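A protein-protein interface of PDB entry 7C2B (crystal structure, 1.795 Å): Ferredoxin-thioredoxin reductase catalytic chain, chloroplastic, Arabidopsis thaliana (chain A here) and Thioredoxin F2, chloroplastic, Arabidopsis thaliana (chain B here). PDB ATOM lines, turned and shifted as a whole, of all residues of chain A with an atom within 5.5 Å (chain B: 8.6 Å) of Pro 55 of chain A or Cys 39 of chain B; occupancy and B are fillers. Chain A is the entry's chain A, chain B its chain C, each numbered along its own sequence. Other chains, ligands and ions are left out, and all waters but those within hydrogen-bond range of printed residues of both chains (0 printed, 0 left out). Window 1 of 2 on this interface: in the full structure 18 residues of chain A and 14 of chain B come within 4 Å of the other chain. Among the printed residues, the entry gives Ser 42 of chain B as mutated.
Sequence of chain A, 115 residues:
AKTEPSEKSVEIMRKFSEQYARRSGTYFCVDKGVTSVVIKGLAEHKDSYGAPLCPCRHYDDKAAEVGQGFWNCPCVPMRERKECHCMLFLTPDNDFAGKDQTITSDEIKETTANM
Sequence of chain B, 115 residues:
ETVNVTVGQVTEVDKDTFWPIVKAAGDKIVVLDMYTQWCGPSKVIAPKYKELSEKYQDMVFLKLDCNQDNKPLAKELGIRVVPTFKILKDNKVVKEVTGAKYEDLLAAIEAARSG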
ATOM      1  N   VAL A  37     -17.274 -16.677 -10.938  1.00  0.00           N
ATOM      2  CA  VAL A  37     -16.703 -17.144  -9.679  1.00  0.00           C
ATOM      3  C   VAL A  37     -15.511 -16.284  -9.278  1.00  0.00           C
ATOM      4  O   VAL A  37     -15.366 -15.899  -8.113  1.00  0.00           O
ATOM      5  CB  VAL A  37     -16.333 -18.634  -9.799  1.00  0.00           C
ATOM      6  CG1 VAL A  37     -15.437 -19.092  -8.648  1.00  0.00           C
ATOM      7  CG2 VAL A  37     -17.607 -19.473  -9.875  1.00  0.00           C
ATOM      8  N   VAL A  38     -14.624 -15.984 -10.231  1.00  0.00           N
ATOM      9  CA  VAL A  38     -13.450 -15.179  -9.901  1.00  0.00           C
ATOM     10  C   VAL A  38     -13.858 -13.759  -9.523  1.00  0.00           C
ATOM     11  O   VAL A  38     -13.310 -13.163  -8.587  1.00  0.00           O
ATOM     12  CB  VAL A  38     -12.454 -15.200 -11.069  1.00  0.00           C
ATOM     13  CG1 VAL A  38     -11.305 -14.206 -10.810  1.00  0.00           C
ATOM     14  CG2 VAL A  38     -11.920 -16.643 -11.264  1.00  0.00           C
ATOM     15  N   GLY A  41     -14.869 -13.843  -6.064  1.00  0.00           N
ATOM     16  CA  GLY A  41     -13.713 -13.962  -5.182  1.00  0.00           C
ATOM     17  C   GLY A  41     -13.002 -12.638  -4.987  1.00  0.00           C
ATOM     18  O   GLY A  41     -12.601 -12.293  -3.868  1.00  0.00           O
ATOM     19  N   LEU A  42     -12.841 -11.876  -6.071  1.00  0.00           N
ATOM     20  CA  LEU A  42     -12.269 -10.544  -5.942  1.00  0.00           C
ATOM     21  C   LEU A  42     -13.120  -9.683  -5.019  1.00  0.00           C
ATOM     22  O   LEU A  42     -12.591  -8.964  -4.162  1.00  0.00           O
ATOM     23  CB  LEU A  42     -12.141  -9.883  -7.318  1.00  0.00           C
ATOM     24  CG  LEU A  42     -11.274 -10.603  -8.348  1.00  0.00           C
ATOM     25  CD1 LEU A  42     -11.388  -9.895  -9.710  1.00  0.00           C
ATOM     26  CD2 LEU A  42      -9.832 -10.650  -7.864  1.00  0.00           C
ATOM     27  N   HIS A  45     -12.733 -10.827  -1.338  1.00  0.00           N
ATOM     28  CA  HIS A  45     -11.468 -10.394  -0.759  1.00  0.00           C
ATOM     29  C   HIS A  45     -11.472  -8.893  -0.497  1.00  0.00           C
ATOM     30  O   HIS A  45     -10.936  -8.434   0.523  1.00  0.00           O
ATOM     31  CB  HIS A  45     -10.308 -10.810  -1.666  1.00  0.00           C
ATOM     32  CG  HIS A  45      -9.935 -12.257  -1.526  1.00  0.00           C
ATOM     33  ND1 HIS A  45      -9.065 -12.893  -2.386  1.00  0.00           N
ATOM     34  CD2 HIS A  45     -10.331 -13.197  -0.630  1.00  0.00           C
ATOM     35  CE1 HIS A  45      -8.919 -14.154  -2.010  1.00  0.00           C
ATOM     36  NE2 HIS A  45      -9.682 -14.367  -0.952  1.00  0.00           N
ATOM     37  N   LEU A  53      -7.426  -9.232  -3.536  1.00  0.00           N
ATOM     38  CA  LEU A  53      -6.343 -10.182  -3.736  1.00  0.00           C
ATOM     39  C   LEU A  53      -6.817 -11.321  -4.626  1.00  0.00           C
ATOM     40  O   LEU A  53      -7.971 -11.752  -4.559  1.00  0.00           O
ATOM     41  CB  LEU A  53      -5.840 -10.748  -2.400  1.00  0.00           C
ATOM     42  CG  LEU A  53      -5.226  -9.739  -1.429  1.00  0.00           C
ATOM     43  CD1 LEU A  53      -4.850 -10.429  -0.134  1.00  0.00           C
ATOM     44  CD2 LEU A  53      -4.009  -9.080  -2.056  1.00  0.00           C
ATOM     45  N   CYS A  54      -5.905 -11.803  -5.455  1.00  0.00           N
ATOM     46  CA  CYS A  54      -6.130 -12.934  -6.336  1.00  0.00           C
ATOM     47  C   CYS A  54      -6.817 -14.063  -5.584  1.00  0.00           C
ATOM     48  O   CYS A  54      -6.298 -14.517  -4.559  1.00  0.00           O
ATOM     49  CB  CYS A  54      -4.808 -13.436  -6.904  1.00  0.00           C
ATOM     50  SG  CYS A  54      -5.102 -14.690  -8.150  1.00  0.00           S
ATOM     51  N   PRO A  55      -7.982 -14.534  -6.046  1.00  0.00           N
ATOM     52  CA  PRO A  55      -8.633 -15.661  -5.368  1.00  0.00           C
ATOM     53  C   PRO A  55      -8.012 -17.009  -5.677  1.00  0.00           C
ATOM     54  O   PRO A  55      -8.439 -18.004  -5.083  1.00  0.00           O
ATOM     55  CB  PRO A  55     -10.087 -15.600  -5.876  1.00  0.00           C
ATOM     56  CG  PRO A  55     -10.020 -14.884  -7.164  1.00  0.00           C
ATOM     57  CD  PRO A  55      -8.827 -13.945  -7.106  1.00  0.00           C
ATOM     58  N   CYS A  56      -7.048 -17.087  -6.589  1.00  0.00           N
ATOM     59  CA  CYS A  56      -6.368 -18.343  -6.878  1.00  0.00           C
ATOM     60  C   CYS A  56      -4.943 -18.343  -6.327  1.00  0.00           C
ATOM     61  O   CYS A  56      -4.030 -18.929  -6.917  1.00  0.00           O
ATOM     62  CB  CYS A  56      -6.380 -18.635  -8.378  1.00  0.00           C
ATOM     63  SG  CYS A  56      -8.048 -19.036  -9.001  1.00  0.00           S
ATOM     64  N   ARG A  57      -4.745 -17.673  -5.196  1.00  0.00           N
ATOM     65  CA  ARG A  57      -3.497 -17.724  -4.445  1.00  0.00           C
ATOM     66  C   ARG A  57      -3.828 -17.944  -2.978  1.00  0.00           C
ATOM     67  O   ARG A  57      -4.904 -17.554  -2.509  1.00  0.00           O
ATOM     68  CB  ARG A  57      -2.681 -16.416  -4.609  1.00  0.00           C
ATOM     69  CG  ARG A  57      -2.268 -16.099  -6.043  1.00  0.00           C
ATOM     70  CD  ARG A  57      -1.164 -17.021  -6.539  1.00  0.00           C
ATOM     71  NE  ARG A  57       0.016 -16.964  -5.684  1.00  0.00           N
ATOM     72  CZ  ARG A  57       1.199 -17.488  -5.993  1.00  0.00           C
ATOM     73  NH1 ARG A  57       1.370 -18.115  -7.148  1.00  0.00           N
ATOM     74  NH2 ARG A  57       2.214 -17.382  -5.146  1.00  0.00           N
ATOM     75  N   TYR A  59      -2.472 -17.103   0.938  1.00  0.00           N
ATOM     76  CA  TYR A  59      -1.683 -16.085   1.613  1.00  0.00           C
ATOM     77  C   TYR A  59      -1.521 -16.402   3.094  1.00  0.00           C
ATOM     78  O   TYR A  59      -2.425 -16.945   3.735  1.00  0.00           O
ATOM     79  CB  TYR A  59      -2.330 -14.709   1.485  1.00  0.00           C
ATOM     80  CG  TYR A  59      -2.761 -14.375   0.083  1.00  0.00           C
ATOM     81  CD1 TYR A  59      -1.824 -14.020  -0.882  1.00  0.00           C
ATOM     82  CD2 TYR A  59      -4.097 -14.424  -0.282  1.00  0.00           C
ATOM     83  CE1 TYR A  59      -2.211 -13.719  -2.184  1.00  0.00           C
ATOM     84  CE2 TYR A  59      -4.495 -14.119  -1.588  1.00  0.00           C
ATOM     85  CZ  TYR A  59      -3.548 -13.759  -2.526  1.00  0.00           C
ATOM     86  OH  TYR A  59      -3.937 -13.444  -3.824  1.00  0.00           O
ATOM     87  N   CYS A  86      -6.085 -17.230 -12.858  1.00  0.00           N
ATOM     88  CA  CYS A  86      -7.485 -17.362 -12.475  1.00  0.00           C
ATOM     89  C   CYS A  86      -8.406 -17.618 -13.659  1.00  0.00           C
ATOM     90  O   CYS A  86      -9.568 -17.972 -13.439  1.00  0.00           O
ATOM     91  CB  CYS A  86      -7.957 -16.082 -11.776  1.00  0.00           C
ATOM     92  SG  CYS A  86      -7.227 -15.877 -10.152  1.00  0.00           S
ATOM     93  N   MET B  34      -6.270 -29.259  -2.890  1.00  0.00           N
ATOM     94  CA  MET B  34      -6.382 -28.077  -2.042  1.00  0.00           C
ATOM     95  C   MET B  34      -6.998 -26.960  -2.870  1.00  0.00           C
ATOM     96  O   MET B  34      -6.432 -26.550  -3.891  1.00  0.00           O
ATOM     97  CB  MET B  34      -5.030 -27.657  -1.474  1.00  0.00           C
ATOM     98  CG  MET B  34      -4.285 -28.816  -0.820  1.00  0.00           C
ATOM     99  SD  MET B  34      -2.600 -28.379  -0.361  1.00  0.00           S
ATOM    100  CE  MET B  34      -2.916 -27.275   1.005  1.00  0.00           C
ATOM    101  N   TYR B  35      -8.172 -26.502  -2.456  1.00  0.00           N
ATOM    102  CA  TYR B  35      -8.963 -25.561  -3.243  1.00  0.00           C
ATOM    103  C   TYR B  35      -9.376 -24.386  -2.373  1.00  0.00           C
ATOM    104  O   TYR B  35      -9.170 -24.381  -1.158  1.00  0.00           O
ATOM    105  CB  TYR B  35     -10.201 -26.242  -3.846  1.00  0.00           C
ATOM    106  CG  TYR B  35     -11.283 -26.641  -2.852  1.00  0.00           C
ATOM    107  CD1 TYR B  35     -11.201 -27.843  -2.140  1.00  0.00           C
ATOM    108  CD2 TYR B  35     -12.403 -25.840  -2.660  1.00  0.00           C
ATOM    109  CE1 TYR B  35     -12.191 -28.212  -1.250  1.00  0.00           C
ATOM    110  CE2 TYR B  35     -13.402 -26.199  -1.772  1.00  0.00           C
ATOM    111  CZ  TYR B  35     -13.306 -27.389  -1.081  1.00  0.00           C
ATOM    112  OH  TYR B  35     -14.306 -27.740  -0.199  1.00  0.00           O
ATOM    113  N   THR B  36      -9.948 -23.370  -3.019  1.00  0.00           N
ATOM    114  CA  THR B  36     -10.653 -22.303  -2.325  1.00  0.00           C
ATOM    115  C   THR B  36     -12.021 -22.111  -2.967  1.00  0.00           C
ATOM    116  O   THR B  36     -12.262 -22.523  -4.108  1.00  0.00           O
ATOM    117  CB  THR B  36      -9.904 -20.952  -2.359  1.00  0.00           C
ATOM    118  OG1 THR B  36      -9.765 -20.520  -3.715  1.00  0.00           O
ATOM    119  CG2 THR B  36      -8.533 -21.062  -1.735  1.00  0.00           C
ATOM    120  N   GLN B  37     -12.900 -21.434  -2.223  1.00  0.00           N
ATOM    121  CA  GLN B  37     -14.301 -21.302  -2.636  1.00  0.00           C
ATOM    122  C   GLN B  37     -14.460 -20.512  -3.930  1.00  0.00           C
ATOM    123  O   GLN B  37     -15.388 -20.782  -4.702  1.00  0.00           O
ATOM    124  CB  GLN B  37     -15.110 -20.650  -1.508  1.00  0.00           C
ATOM    125  CG  GLN B  37     -16.617 -20.473  -1.778  1.00  0.00           C
ATOM    126  CD  GLN B  37     -17.314 -19.598  -0.729  1.00  0.00           C
ATOM    127  OE1 GLN B  37     -16.709 -19.201   0.275  1.00  0.00           O
ATOM    128  NE2 GLN B  37     -18.593 -19.295  -0.960  1.00  0.00           N
ATOM    129  N   TRP B  38     -13.580 -19.547  -4.204  1.00  0.00           N
ATOM    130  CA  TRP B  38     -13.814 -18.643  -5.327  1.00  0.00           C
ATOM    131  C   TRP B  38     -12.723 -18.693  -6.396  1.00  0.00           C
ATOM    132  O   TRP B  38     -12.593 -17.750  -7.180  1.00  0.00           O
ATOM    133  CB  TRP B  38     -13.976 -17.210  -4.820  1.00  0.00           C
ATOM    134  CG  TRP B  38     -15.162 -16.995  -3.926  1.00  0.00           C
ATOM    135  CD1 TRP B  38     -15.141 -16.612  -2.611  1.00  0.00           C
ATOM    136  CD2 TRP B  38     -16.545 -17.145  -4.278  1.00  0.00           C
ATOM    137  NE1 TRP B  38     -16.426 -16.517  -2.127  1.00  0.00           N
ATOM    138  CE2 TRP B  38     -17.305 -16.841  -3.128  1.00  0.00           C
ATOM    139  CE3 TRP B  38     -17.216 -17.510  -5.454  1.00  0.00           C
ATOM    140  CZ2 TRP B  38     -18.704 -16.886  -3.119  1.00  0.00           C
ATOM    141  CZ3 TRP B  38     -18.610 -17.554  -5.443  1.00  0.00           C
ATOM    142  CH2 TRP B  38     -19.334 -17.248  -4.282  1.00  0.00           C
ATOM    143  N   CYS B  39     -11.935 -19.764  -6.462  1.00  0.00           N
ATOM    144  CA  CYS B  39     -10.939 -19.905  -7.518  1.00  0.00           C
ATOM    145  C   CYS B  39     -11.602 -20.599  -8.705  1.00  0.00           C
ATOM    146  O   CYS B  39     -11.918 -21.789  -8.636  1.00  0.00           O
ATOM    147  CB  CYS B  39      -9.719 -20.691  -7.023  1.00  0.00           C
ATOM    148  SG  CYS B  39      -8.451 -20.940  -8.304  1.00  0.00           S
ATOM    149  N   GLY B  40     -11.823 -19.855  -9.791  1.00  0.00           N
ATOM    150  CA  GLY B  40     -12.467 -20.390 -10.973  1.00  0.00           C
ATOM    151  C   GLY B  40     -11.911 -21.733 -11.444  1.00  0.00           C
ATOM    152  O   GLY B  40     -12.646 -22.720 -11.570  1.00  0.00           O
ATOM    153  N   PRO B  41     -10.604 -21.784 -11.726  1.00  0.00           N
ATOM    154  CA  PRO B  41     -10.011 -23.032 -12.232  1.00  0.00           C
ATOM    155  C   PRO B  41     -10.149 -24.213 -11.280  1.00  0.00           C
ATOM    156  O   PRO B  41     -10.199 -25.354 -11.750  1.00  0.00           O
ATOM    157  CB  PRO B  41      -8.540 -22.658 -12.455  1.00  0.00           C
ATOM    158  CG  PRO B  41      -8.552 -21.140 -12.622  1.00  0.00           C
ATOM    159  CD  PRO B  41      -9.661 -20.648 -11.777  1.00  0.00           C
ATOM    160  N   SER B  42     -10.219 -23.975  -9.969  1.00  0.00           N
ATOM    161  CA  SER B  42     -10.537 -25.051  -9.034  1.00  0.00           C
ATOM    162  C   SER B  42     -11.842 -25.725  -9.413  1.00  0.00           C
ATOM    163  O   SER B  42     -11.948 -26.954  -9.406  1.00  0.00           O
ATOM    164  CB  SER B  42     -10.656 -24.514  -7.612  1.00  0.00           C
ATOM    165  OG  SER B  42      -9.423 -24.528  -6.960  1.00  0.00           O
ATOM    166  N   LYS B  43     -12.864 -24.917  -9.708  1.00  0.00           N
ATOM    167  CA  LYS B  43     -14.173 -25.456 -10.034  1.00  0.00           C
ATOM    168  C   LYS B  43     -14.162 -26.145 -11.391  1.00  0.00           C
ATOM    169  O   LYS B  43     -14.915 -27.100 -11.599  1.00  0.00           O
ATOM    170  CB  LYS B  43     -15.220 -24.331  -9.975  1.00  0.00           C
ATOM    171  CG  LYS B  43     -15.498 -23.870  -8.533  1.00  0.00           C
ATOM    172  CD  LYS B  43     -16.742 -23.015  -8.421  1.00  0.00           C
ATOM    173  CE  LYS B  43     -16.911 -22.480  -7.011  1.00  0.00           C
ATOM    174  NZ  LYS B  43     -16.766 -23.566  -5.992  1.00  0.00           N
ATOM    175  N   VAL B  44     -13.298 -25.705 -12.305  1.00  0.00           N
ATOM    176  CA  VAL B  44     -13.172 -26.366 -13.600  1.00  0.00           C
ATOM    177  C   VAL B  44     -12.613 -27.775 -13.430  1.00  0.00           C
ATOM    178  O   VAL B  44     -13.119 -28.743 -14.018  1.00  0.00           O
ATOM    179  CB  VAL B  44     -12.284 -25.535 -14.542  1.00  0.00           C
ATOM    180  CG1 VAL B  44     -12.043 -26.281 -15.840  1.00  0.00           C
ATOM    181  CG2 VAL B  44     -12.922 -24.180 -14.826  1.00  0.00           C
ATOM    182  N   ILE B  45     -11.548 -27.917 -12.639  1.00  0.00           N
ATOM    183  CA  ILE B  45     -10.920 -29.233 -12.555  1.00  0.00           C
ATOM    184  C   ILE B  45     -11.642 -30.151 -11.573  1.00  0.00           C
ATOM    185  O   ILE B  45     -11.443 -31.376 -11.623  1.00  0.00           O
ATOM    186  CB  ILE B  45      -9.423 -29.091 -12.219  1.00  0.00           C
ATOM    187  CG1 ILE B  45      -8.663 -30.404 -12.491  1.00  0.00           C
ATOM    188  CG2 ILE B  45      -9.214 -28.642 -10.789  1.00  0.00           C
ATOM    189  CD1 ILE B  45      -7.178 -30.198 -12.604  1.00  0.00           C
ATOM    190  N   ALA B  46     -12.489 -29.610 -10.695  1.00  0.00           N
ATOM    191  CA  ALA B  46     -13.149 -30.435  -9.681  1.00  0.00           C
ATOM    192  C   ALA B  46     -13.898 -31.643 -10.243  1.00  0.00           C
ATOM    193  O   ALA B  46     -13.742 -32.747  -9.687  1.00  0.00           O
ATOM    194  CB  ALA B  46     -14.086 -29.561  -8.835  1.00  0.00           C
ATOM    195  N   ASP B  65     -10.681 -27.457   1.681  1.00  0.00           N
ATOM    196  CA  ASP B  65     -10.968 -26.039   1.465  1.00  0.00           C
ATOM    197  C   ASP B  65      -9.967 -25.226   2.277  1.00  0.00           C
ATOM    198  O   ASP B  65      -9.993 -25.260   3.508  1.00  0.00           O
ATOM    199  CB  ASP B  65     -12.412 -25.744   1.874  1.00  0.00           C
ATOM    200  CG  ASP B  65     -12.836 -24.303   1.619  1.00  0.00           C
ATOM    201  OD1 ASP B  65     -11.986 -23.446   1.274  1.00  0.00           O
ATOM    202  OD2 ASP B  65     -14.053 -24.025   1.773  1.00  0.00           O
ATOM    203  N   CYS B  66      -9.068 -24.513   1.598  1.00  0.00           N
ATOM    204  CA  CYS B  66      -8.038 -23.723   2.276  1.00  0.00           C
ATOM    205  C   CYS B  66      -8.598 -22.355   2.679  1.00  0.00           C
ATOM    206  O   CYS B  66      -8.294 -21.314   2.097  1.00  0.00           O
ATOM    207  CB  CYS B  66      -6.796 -23.614   1.402  1.00  0.00           C
ATOM    208  SG  CYS B  66      -6.050 -25.253   1.088  1.00  0.00           S
ATOM    209  N   ARG B  80       0.733 -22.218  -2.325  1.00  0.00           N
ATOM    210  CA  ARG B  80       0.805 -20.848  -2.824  1.00  0.00           C
ATOM    211  C   ARG B  80      -0.119 -20.678  -4.026  1.00  0.00           C
ATOM    212  O   ARG B  80      -0.894 -19.726  -4.086  1.00  0.00           O
ATOM    213  CB  ARG B  80       2.253 -20.491  -3.187  1.00  0.00           C
ATOM    214  CG  ARG B  80       3.157 -20.228  -1.959  1.00  0.00           C
ATOM    215  CD  ARG B  80       2.627 -19.013  -1.178  1.00  0.00           C
ATOM    216  NE  ARG B  80       3.414 -18.637   0.003  1.00  0.00           N
ATOM    217  CZ  ARG B  80       3.025 -18.855   1.260  1.00  0.00           C
ATOM    218  NH1 ARG B  80       3.786 -18.469   2.277  1.00  0.00           N
ATOM    219  NH2 ARG B  80       1.874 -19.473   1.504  1.00  0.00           N
ATOM    220  N   VAL B  81      -0.046 -21.595  -4.976  1.00  0.00           N
ATOM    221  CA  VAL B  81      -0.929 -21.631  -6.139  1.00  0.00           C
ATOM    222  C   VAL B  81      -2.201 -22.385  -5.779  1.00  0.00           C
ATOM    223  O   VAL B  81      -2.153 -23.425  -5.112  1.00  0.00           O
ATOM    224  CB  VAL B  81      -0.216 -22.300  -7.330  1.00  0.00           C
ATOM    225  CG1 VAL B  81      -1.117 -22.331  -8.580  1.00  0.00           C
ATOM    226  CG2 VAL B  81       1.096 -21.598  -7.611  1.00  0.00           C
ATOM    227  N   VAL B  82      -3.346 -21.881  -6.218  1.00  0.00           N
ATOM    228  CA  VAL B  82      -4.614 -22.604  -6.120  1.00  0.00           C
ATOM    229  C   VAL B  82      -5.066 -22.927  -7.540  1.00  0.00           C
ATOM    230  O   VAL B  82      -5.097 -22.026  -8.380  1.00  0.00           O
ATOM    231  CB  VAL B  82      -5.687 -21.781  -5.383  1.00  0.00           C
ATOM    232  CG1 VAL B  82      -6.959 -22.617  -5.139  1.00  0.00           C
ATOM    233  CG2 VAL B  82      -5.115 -21.190  -4.087  1.00  0.00           C
ATOM    234  N   PRO B  83      -5.401 -24.190  -7.863  1.00  0.00           N
ATOM    235  CA  PRO B  83      -5.282 -25.354  -6.979  1.00  0.00           C
ATOM    236  C   PRO B  83      -3.874 -25.834  -6.800  1.00  0.00           C
ATOM    237  O   PRO B  83      -2.991 -25.564  -7.619  1.00  0.00           O
ATOM    238  CB  PRO B  83      -6.081 -26.445  -7.702  1.00  0.00           C
ATOM    239  CG  PRO B  83      -6.183 -26.003  -9.102  1.00  0.00           C
ATOM    240  CD  PRO B  83      -6.148 -24.505  -9.092  1.00  0.00           C
ATOM    241  N   THR B  84      -3.677 -26.581  -5.722  1.00  0.00           N
ATOM    242  CA  THR B  84      -2.494 -27.404  -5.563  1.00  0.00           C
ATOM    243  C   THR B  84      -2.943 -28.812  -5.207  1.00  0.00           C
ATOM    244  O   THR B  84      -3.868 -28.991  -4.413  1.00  0.00           O
ATOM    245  CB  THR B  84      -1.555 -26.840  -4.498  1.00  0.00           C
ATOM    246  OG1 THR B  84      -0.898 -25.686  -5.035  1.00  0.00           O
ATOM    247  CG2 THR B  84      -0.482 -27.880  -4.115  1.00  0.00           C
ATOM    248  N   GLY B  99      -1.565 -25.738  -9.882  1.00  0.00           N
ATOM    249  CA  GLY B  99      -2.368 -25.294 -11.009  1.00  0.00           C
ATOM    250  C   GLY B  99      -3.459 -26.275 -11.381  1.00  0.00           C
ATOM    251  O   GLY B  99      -3.564 -27.382 -10.849  1.00  0.00           O
ATOM    252  N   ALA B 100      -4.279 -25.873 -12.340  1.00  0.00           N
ATOM    253  CA  ALA B 100      -5.424 -26.683 -12.766  1.00  0.00           C
ATOM    254  C   ALA B 100      -5.077 -27.483 -14.011  1.00  0.00           C
ATOM    255  O   ALA B 100      -5.779 -27.481 -15.014  1.00  0.00           O
ATOM    256  CB  ALA B 100      -6.646 -25.801 -12.989  1.00  0.00           C
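Of the 12 printed residues of chain A, 7 touch a printed residue of chain B.
Hydrophobic or aromatic side chains of chain A that line the printed part of chain B: Val 37, Val 38 and Pro 55.
Hydrophobic or aromatic side chains of chain B that line the printed part of chain A: Trp 38, Pro 41, Val 81 and Val 82.
Along chain B the printed residues that touch a printed residue of chain A span positions 36 to 82.
Printed residues of chain B within 4 Å of Gly 41 of chain A: Trp 38 (3.3 Å).
Leu 42 of chain A touches none of the printed residues of chain B.
Pro 55 of chain A touches just these residues of chain B: Thr 36, Trp 38 and Cys 39.
Tyr 59 of chain A touches none of the printed residues of chain B.
Of the printed residues of chain A, Gly 40 of chain B touches Val 37 (3.9 Å), Val 38 (3.5 Å) and Cys 56 (3.9 Å).
Printed residues of chain A within 4 Å of Pro 41 of chain B: Cys 56 (3.6 Å) and Cys 86 (3.2 Å).
Of the printed residues of chain A, Val 81 of chain B touches Arg 57 (3.5 Å).
Among the printed residues, pairs that only touch across the chains: Val 37 of chain A with Gly 40 of chain B (3.9 Å), Val 37 of chain A with Lys 43 of chain B (3.9 Å), Val 38 of chain A with Trp 38 of chain B (3.8 Å), Val 38 of chain A with Gly 40 of chain B (3.5 Å), Gly 41 of chain A with Trp 38 of chain B (3.3 Å), Pro 55 of chain A with Trp 38 of chain B (3.6 Å), Pro 55 of chain A with Cys 39 of chain B (3.6 Å), Cys 56 of chain A with Gly 40 of chain B (3.9 Å), Cys 56 of chain A with Pro 41 of chain B (3.6 Å), Arg 57 of chain A with Val 81 of chain B (3.5 Å), Arg 57 of chain A with Val 82 of chain B (3.7 Å) and Cys 86 of chain A with Pro 41 of chain B (3.2 Å).
N of Cys 56 of chain A sits close to SG of Cys 54 of chain A (3.5 Å).
SG of Cys 86 of chain A lies close to SG of Cys 56 of chain A (3.5 Å).
The backbone carbonyl oxygen (O) of Gln 37 of chain B sits close to the side-chain amino group (NZ) of Lys 43 of chain B (3.4 Å).
O of Val 81 of chain B sits at hydrogen-bond distance from OG1 of Thr 84 of chain B (2.6 Å).
The backbone carbonyl oxygen (O) of Pro 55 of chain A is in hydrogen-bond range of the side-chain hydroxyl (OG1) of Thr 36 of chain B (3.2 Å).
SG of Cys 39 of chain B is disulfide-bonded to SG of Cys 56 of chain A (2.1 Å).
The backbone carbonyl oxygen (O) of Cys 56 of chain A lies within hydrogen-bond range of the backbone NH (N) of Val 82 of chain B, at 3.1 Å.
NE of Arg 57 of chain A lies close to O of Arg 80 of chain B (3.3 Å).
The backbone carbonyl oxygen (O) of Val 37 of chain A sits close to the backbone carbonyl oxygen (O) of Trp 38 of chain B.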
